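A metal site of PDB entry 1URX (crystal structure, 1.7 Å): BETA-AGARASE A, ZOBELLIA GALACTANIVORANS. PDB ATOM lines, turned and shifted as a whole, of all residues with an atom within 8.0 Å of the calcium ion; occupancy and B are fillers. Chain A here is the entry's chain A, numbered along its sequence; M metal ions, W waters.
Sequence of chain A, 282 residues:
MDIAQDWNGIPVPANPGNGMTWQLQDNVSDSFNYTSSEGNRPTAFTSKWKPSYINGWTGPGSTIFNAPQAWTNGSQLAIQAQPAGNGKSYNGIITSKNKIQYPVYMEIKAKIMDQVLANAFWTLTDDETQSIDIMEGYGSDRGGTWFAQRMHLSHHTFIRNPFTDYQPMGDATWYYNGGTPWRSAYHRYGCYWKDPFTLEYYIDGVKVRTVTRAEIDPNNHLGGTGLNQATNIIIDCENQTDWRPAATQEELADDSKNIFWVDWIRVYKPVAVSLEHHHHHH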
ATOM      1  N   GLN A   5      28.791 -19.033 -32.268  1.00  0.00           N
ATOM      2  CA  GLN A   5      29.075 -18.437 -30.918  1.00  0.00           C
ATOM      3  C   GLN A   5      29.048 -16.905 -30.901  1.00  0.00           C
ATOM      4  O   GLN A   5      29.231 -16.244 -31.924  1.00  0.00           O
ATOM      5  CB  GLN A   5      30.473 -18.902 -30.435  1.00  0.00           C
ATOM      6  CG  GLN A   5      30.726 -20.435 -30.459  1.00  0.00           C
ATOM      7  CD  GLN A   5      30.171 -21.188 -29.265  1.00  0.00           C
ATOM      8  OE1 GLN A   5      30.514 -22.361 -29.041  1.00  0.00           O
ATOM      9  NE2 GLN A   5      29.319 -20.537 -28.506  1.00  0.00           N
ATOM     10  N   ASP A   6      28.869 -16.314 -29.712  1.00  0.00           N
ATOM     11  CA  ASP A   6      28.783 -14.863 -29.582  1.00  0.00           C
ATOM     12  C   ASP A   6      29.976 -14.097 -30.110  1.00  0.00           C
ATOM     13  O   ASP A   6      29.821 -12.978 -30.578  1.00  0.00           O
ATOM     14  CB  ASP A   6      28.603 -14.453 -28.116  1.00  0.00           C
ATOM     15  CG  ASP A   6      27.340 -14.974 -27.529  1.00  0.00           C
ATOM     16  OD1 ASP A   6      27.283 -15.035 -26.284  1.00  0.00           O
ATOM     17  OD2 ASP A   6      26.345 -15.334 -28.243  1.00  0.00           O
ATOM     18  N   TRP A   7      31.143 -14.702 -29.993  1.00  0.00           N
ATOM     19  CA  TRP A   7      32.396 -14.073 -30.403  1.00  0.00           C
ATOM     20  C   TRP A   7      32.770 -14.318 -31.872  1.00  0.00           C
ATOM     21  O   TRP A   7      33.845 -13.943 -32.320  1.00  0.00           O
ATOM     22  CB  TRP A   7      33.519 -14.606 -29.485  1.00  0.00           C
ATOM     23  CG  TRP A   7      33.666 -16.076 -29.530  1.00  0.00           C
ATOM     24  CD1 TRP A   7      34.327 -16.819 -30.494  1.00  0.00           C
ATOM     25  CD2 TRP A   7      33.181 -17.013 -28.577  1.00  0.00           C
ATOM     26  NE1 TRP A   7      34.239 -18.148 -30.194  1.00  0.00           N
ATOM     27  CE2 TRP A   7      33.553 -18.305 -29.024  1.00  0.00           C
ATOM     28  CE3 TRP A   7      32.440 -16.906 -27.392  1.00  0.00           C
ATOM     29  CZ2 TRP A   7      33.246 -19.444 -28.327  1.00  0.00           C
ATOM     30  CZ3 TRP A   7      32.134 -18.029 -26.711  1.00  0.00           C
ATOM     31  CH2 TRP A   7      32.534 -19.292 -27.165  1.00  0.00           C
ATOM     32  N   ASP A  30      32.160 -21.079 -23.609  1.00  0.00           N
ATOM     33  CA  ASP A  30      30.698 -21.105 -23.442  1.00  0.00           C
ATOM     34  C   ASP A  30      30.124 -19.717 -23.785  1.00  0.00           C
ATOM     35  O   ASP A  30      30.640 -18.672 -23.348  1.00  0.00           O
ATOM     36  CB  ASP A  30      30.361 -21.511 -22.023  1.00  0.00           C
ATOM     37  CG  ASP A  30      28.966 -22.111 -21.896  1.00  0.00           C
ATOM     38  OD1 ASP A  30      28.684 -22.787 -20.879  1.00  0.00           O
ATOM     39  OD2 ASP A  30      28.114 -21.930 -22.772  1.00  0.00           O
ATOM     40  N   SER A  31      29.094 -19.692 -24.642  1.00  0.00           N
ATOM     41  CA  SER A  31      28.362 -18.455 -24.908  1.00  0.00           C
ATOM     42  C   SER A  31      27.244 -18.234 -23.875  1.00  0.00           C
ATOM     43  O   SER A  31      26.642 -17.165 -23.866  1.00  0.00           O
ATOM     44  CB  SER A  31      27.725 -18.444 -26.303  1.00  0.00           C
ATOM     45  OG  SER A  31      28.680 -18.197 -27.314  1.00  0.00           O
ATOM     46  N   PHE A  32      26.998 -19.230 -23.034  1.00  0.00           N
ATOM     47  CA  PHE A  32      26.004 -19.192 -21.935  1.00  0.00           C
ATOM     48  C   PHE A  32      24.590 -18.875 -22.462  1.00  0.00           C
ATOM     49  O   PHE A  32      23.754 -18.289 -21.757  1.00  0.00           O
ATOM     50  CB  PHE A  32      26.398 -18.186 -20.820  1.00  0.00           C
ATOM     51  CG  PHE A  32      27.730 -18.523 -20.149  1.00  0.00           C
ATOM     52  CD1 PHE A  32      28.826 -17.670 -20.260  1.00  0.00           C
ATOM     53  CD2 PHE A  32      27.855 -19.667 -19.404  1.00  0.00           C
ATOM     54  CE1 PHE A  32      30.023 -18.004 -19.636  1.00  0.00           C
ATOM     55  CE2 PHE A  32      29.049 -19.995 -18.767  1.00  0.00           C
ATOM     56  CZ  PHE A  32      30.118 -19.164 -18.890  1.00  0.00           C
ATOM     57  N   ASN A  33      24.324 -19.256 -23.711  1.00  0.00           N
ATOM     58  CA  ASN A  33      23.037 -18.955 -24.315  1.00  0.00           C
ATOM     59  C   ASN A  33      22.012 -20.053 -24.016  1.00  0.00           C
ATOM     60  O   ASN A  33      21.462 -20.704 -24.935  1.00  0.00           O
ATOM     61  CB  ASN A  33      23.214 -18.709 -25.821  1.00  0.00           C
ATOM     62  CG  ASN A  33      24.048 -17.472 -26.123  1.00  0.00           C
ATOM     63  OD1 ASN A  33      24.200 -16.529 -25.294  1.00  0.00           O
ATOM     64  ND2 ASN A  33      24.594 -17.456 -27.328  1.00  0.00           N
ATOM     65  N   TYR A  34      21.793 -20.268 -22.718  1.00  0.00           N
ATOM     66  CA  TYR A  34      20.826 -21.207 -22.195  1.00  0.00           C
ATOM     67  C   TYR A  34      20.387 -20.752 -20.807  1.00  0.00           C
ATOM     68  O   TYR A  34      21.048 -19.933 -20.135  1.00  0.00           O
ATOM     69  CB  TYR A  34      21.381 -22.636 -22.147  1.00  0.00           C
ATOM     70  CG  TYR A  34      22.731 -22.716 -21.466  1.00  0.00           C
ATOM     71  CD1 TYR A  34      22.827 -22.845 -20.100  1.00  0.00           C
ATOM     72  CD2 TYR A  34      23.903 -22.662 -22.211  1.00  0.00           C
ATOM     73  CE1 TYR A  34      24.078 -22.896 -19.463  1.00  0.00           C
ATOM     74  CE2 TYR A  34      25.166 -22.720 -21.576  1.00  0.00           C
ATOM     75  CZ  TYR A  34      25.223 -22.867 -20.210  1.00  0.00           C
ATOM     76  OH  TYR A  34      26.431 -22.936 -19.542  1.00  0.00           O
ATOM     77  N   ASN A  73      20.704 -16.949 -17.821  1.00  0.00           N
ATOM     78  CA  ASN A  73      19.374 -16.350 -18.130  1.00  0.00           C
ATOM     79  C   ASN A  73      18.977 -16.465 -19.596  1.00  0.00           C
ATOM     80  O   ASN A  73      18.085 -15.746 -20.058  1.00  0.00           O
ATOM     81  CB  ASN A  73      19.337 -14.866 -17.693  1.00  0.00           C
ATOM     82  CG  ASN A  73      20.204 -13.985 -18.569  1.00  0.00           C
ATOM     83  OD1 ASN A  73      20.859 -14.486 -19.489  1.00  0.00           O
ATOM     84  ND2 ASN A  73      20.242 -12.672 -18.282  1.00  0.00           N
ATOM     85  N   GLY A  74      19.618 -17.346 -20.324  1.00  0.00           N
ATOM     86  CA  GLY A  74      19.354 -17.530 -21.736  1.00  0.00           C
ATOM     87  C   GLY A  74      20.351 -16.843 -22.636  1.00  0.00           C
ATOM     88  O   GLY A  74      20.432 -17.168 -23.804  1.00  0.00           O
ATOM     89  N   SER A  75      21.141 -15.911 -22.102  1.00  0.00           N
ATOM     90  CA  SER A  75      22.169 -15.243 -22.866  1.00  0.00           C
ATOM     91  C   SER A  75      23.470 -15.002 -22.053  1.00  0.00           C
ATOM     92  O   SER A  75      24.521 -14.899 -22.656  1.00  0.00           O
ATOM     93  CB  SER A  75      21.684 -13.925 -23.460  1.00  0.00           C
ATOM     94  OG  SER A  75      21.282 -13.007 -22.467  1.00  0.00           O
ATOM     95  N   GLN A  76      23.379 -14.892 -20.729  1.00  0.00           N
ATOM     96  CA  GLN A  76      24.543 -14.579 -19.885  1.00  0.00           C
ATOM     97  C   GLN A  76      24.586 -15.405 -18.607  1.00  0.00           C
ATOM     98  O   GLN A  76      23.545 -15.847 -18.072  1.00  0.00           O
ATOM     99  CB  GLN A  76      24.534 -13.098 -19.552  1.00  0.00           C
ATOM    100  CG  GLN A  76      24.482 -12.244 -20.789  1.00  0.00           C
ATOM    101  CD  GLN A  76      24.721 -10.808 -20.574  1.00  0.00           C
ATOM    102  OE1 GLN A  76      24.548 -10.013 -21.514  1.00  0.00           O
ATOM    103  NE2 GLN A  76      25.031 -10.422 -19.350  1.00  0.00           N
ATOM    104  N   LEU A  77      25.806 -15.609 -18.103  1.00  0.00           N
ATOM    105  CA  LEU A  77      26.050 -16.133 -16.789  1.00  0.00           C
ATOM    106  C   LEU A  77      25.916 -14.984 -15.800  1.00  0.00           C
ATOM    107  O   LEU A  77      26.506 -13.934 -16.027  1.00  0.00           O
ATOM    108  CB  LEU A  77      27.455 -16.728 -16.706  1.00  0.00           C
ATOM    109  CG  LEU A  77      27.984 -17.131 -15.348  1.00  0.00           C
ATOM    110  CD1 LEU A  77      27.344 -18.409 -14.889  1.00  0.00           C
ATOM    111  CD2 LEU A  77      29.528 -17.313 -15.366  1.00  0.00           C
ATOM    112  N   LYS A 109      33.826 -11.689 -21.943  1.00  0.00           N
ATOM    113  CA  LYS A 109      33.148 -10.405 -22.069  1.00  0.00           C
ATOM    114  C   LYS A 109      32.216 -10.293 -20.840  1.00  0.00           C
ATOM    115  O   LYS A 109      31.370 -11.129 -20.650  1.00  0.00           O
ATOM    116  CB  LYS A 109      32.311 -10.314 -23.361  1.00  0.00           C
ATOM    117  CG  LYS A 109      31.484  -9.068 -23.421  1.00  0.00           C
ATOM    118  CD  LYS A 109      30.615  -9.061 -24.704  1.00  0.00           C
ATOM    119  CE  LYS A 109      29.559  -8.003 -24.645  1.00  0.00           C
ATOM    120  NZ  LYS A 109      28.423  -8.373 -25.560  1.00  0.00           N
ATOM    121  N   VAL A 262      28.527 -12.207 -17.182  1.00  0.00           N
ATOM    122  CA  VAL A 262      29.496 -12.727 -18.137  1.00  0.00           C
ATOM    123  C   VAL A 262      28.710 -13.204 -19.373  1.00  0.00           C
ATOM    124  O   VAL A 262      28.014 -14.186 -19.305  1.00  0.00           O
ATOM    125  CB  VAL A 262      30.322 -13.897 -17.547  1.00  0.00           C
ATOM    126  CG1 VAL A 262      31.335 -14.411 -18.592  1.00  0.00           C
ATOM    127  CG2 VAL A 262      31.024 -13.463 -16.262  1.00  0.00           C
ATOM    128  N   ASP A 263      28.825 -12.474 -20.475  1.00  0.00           N
ATOM    129  CA  ASP A 263      28.173 -12.858 -21.726  1.00  0.00           C
ATOM    130  C   ASP A 263      28.749 -14.111 -22.339  1.00  0.00           C
ATOM    131  O   ASP A 263      28.018 -14.917 -22.960  1.00  0.00           O
ATOM    132  CB  ASP A 263      28.300 -11.717 -22.710  1.00  0.00           C
ATOM    133  CG  ASP A 263      27.333 -11.796 -23.886  1.00  0.00           C
ATOM    134  OD1 ASP A 263      26.420 -12.622 -23.915  1.00  0.00           O
ATOM    135  OD2 ASP A 263      27.455 -10.993 -24.822  1.00  0.00           O
ATOM    136  N   TRP A 264      30.067 -14.283 -22.219  1.00  0.00           N
ATOM    137  CA  TRP A 264      30.724 -15.434 -22.775  1.00  0.00           C
ATOM    138  C   TRP A 264      32.140 -15.572 -22.269  1.00  0.00           C
ATOM    139  O   TRP A 264      32.730 -14.591 -21.793  1.00  0.00           O
ATOM    140  CB  TRP A 264      30.712 -15.364 -24.302  1.00  0.00           C
ATOM    141  CG  TRP A 264      31.094 -14.082 -25.003  1.00  0.00           C
ATOM    142  CD1 TRP A 264      30.240 -13.189 -25.579  1.00  0.00           C
ATOM    143  CD2 TRP A 264      32.416 -13.629 -25.331  1.00  0.00           C
ATOM    144  NE1 TRP A 264      30.942 -12.224 -26.252  1.00  0.00           N
ATOM    145  CE2 TRP A 264      32.278 -12.443 -26.083  1.00  0.00           C
ATOM    146  CE3 TRP A 264      33.700 -14.081 -25.038  1.00  0.00           C
ATOM    147  CZ2 TRP A 264      33.378 -11.717 -26.572  1.00  0.00           C
ATOM    148  CZ3 TRP A 264      34.784 -13.364 -25.479  1.00  0.00           C
ATOM    149  CH2 TRP A 264      34.629 -12.182 -26.256  1.00  0.00           C
ATOM    150  N   ILE A 265      32.646 -16.790 -22.395  1.00  0.00           N
ATOM    151  CA  ILE A 265      34.068 -17.090 -22.129  1.00  0.00           C
ATOM    152  C   ILE A 265      34.580 -17.840 -23.369  1.00  0.00           C
ATOM    153  O   ILE A 265      33.893 -18.731 -23.877  1.00  0.00           O
ATOM    154  CB  ILE A 265      34.259 -17.908 -20.831  1.00  0.00           C
ATOM    155  CG1 ILE A 265      35.749 -18.261 -20.629  1.00  0.00           C
ATOM    156  CG2 ILE A 265      33.456 -19.231 -20.792  1.00  0.00           C
ATOM    157  CD1 ILE A 265      36.096 -18.801 -19.245  1.00  0.00           C
HETATM  158 CA    CA M   1      25.970 -14.991 -24.332  1.00  0.00          CA
HETATM  159  O   HOH W   1      24.444 -13.650 -25.785  1.00  0.00           O
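Within 4 Å of the calcium ion: Asp 6, Ser 31, Asn 33, Ser 75 and Asp 263.
The nearest printed residue that does not touch the calcium ion is Gln 76 (4.4 Å).
The side-chain amino group (NZ) of Lys 109 lies within salt-bridge range of the side-chain carboxylate (OD2) of Asp 263, at 2.9 Å.
The side-chain amide oxygen of Asn 73 sits at hydrogen-bond distance from the backbone NH of Ser 75, at 3.0 Å.
The side-chain hydroxyl (OG) of Ser 31 is in hydrogen-bond range of the side-chain amide nitrogen (NE2) of Gln 5 (2.7 Å).
The calcium ion is bound by O of Ser 75 (2.2 Å), O of Ser 31 (2.3 Å), OD1 of Asp 6 (2.4 Å), OD1 of Asp 263 (2.4 Å), O of Asp 263 (2.5 Å), water W1 (2.5 Å) and OD1 of Asn 33 (2.5 Å).
The calcium ion has seven donor atoms within binding distance.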
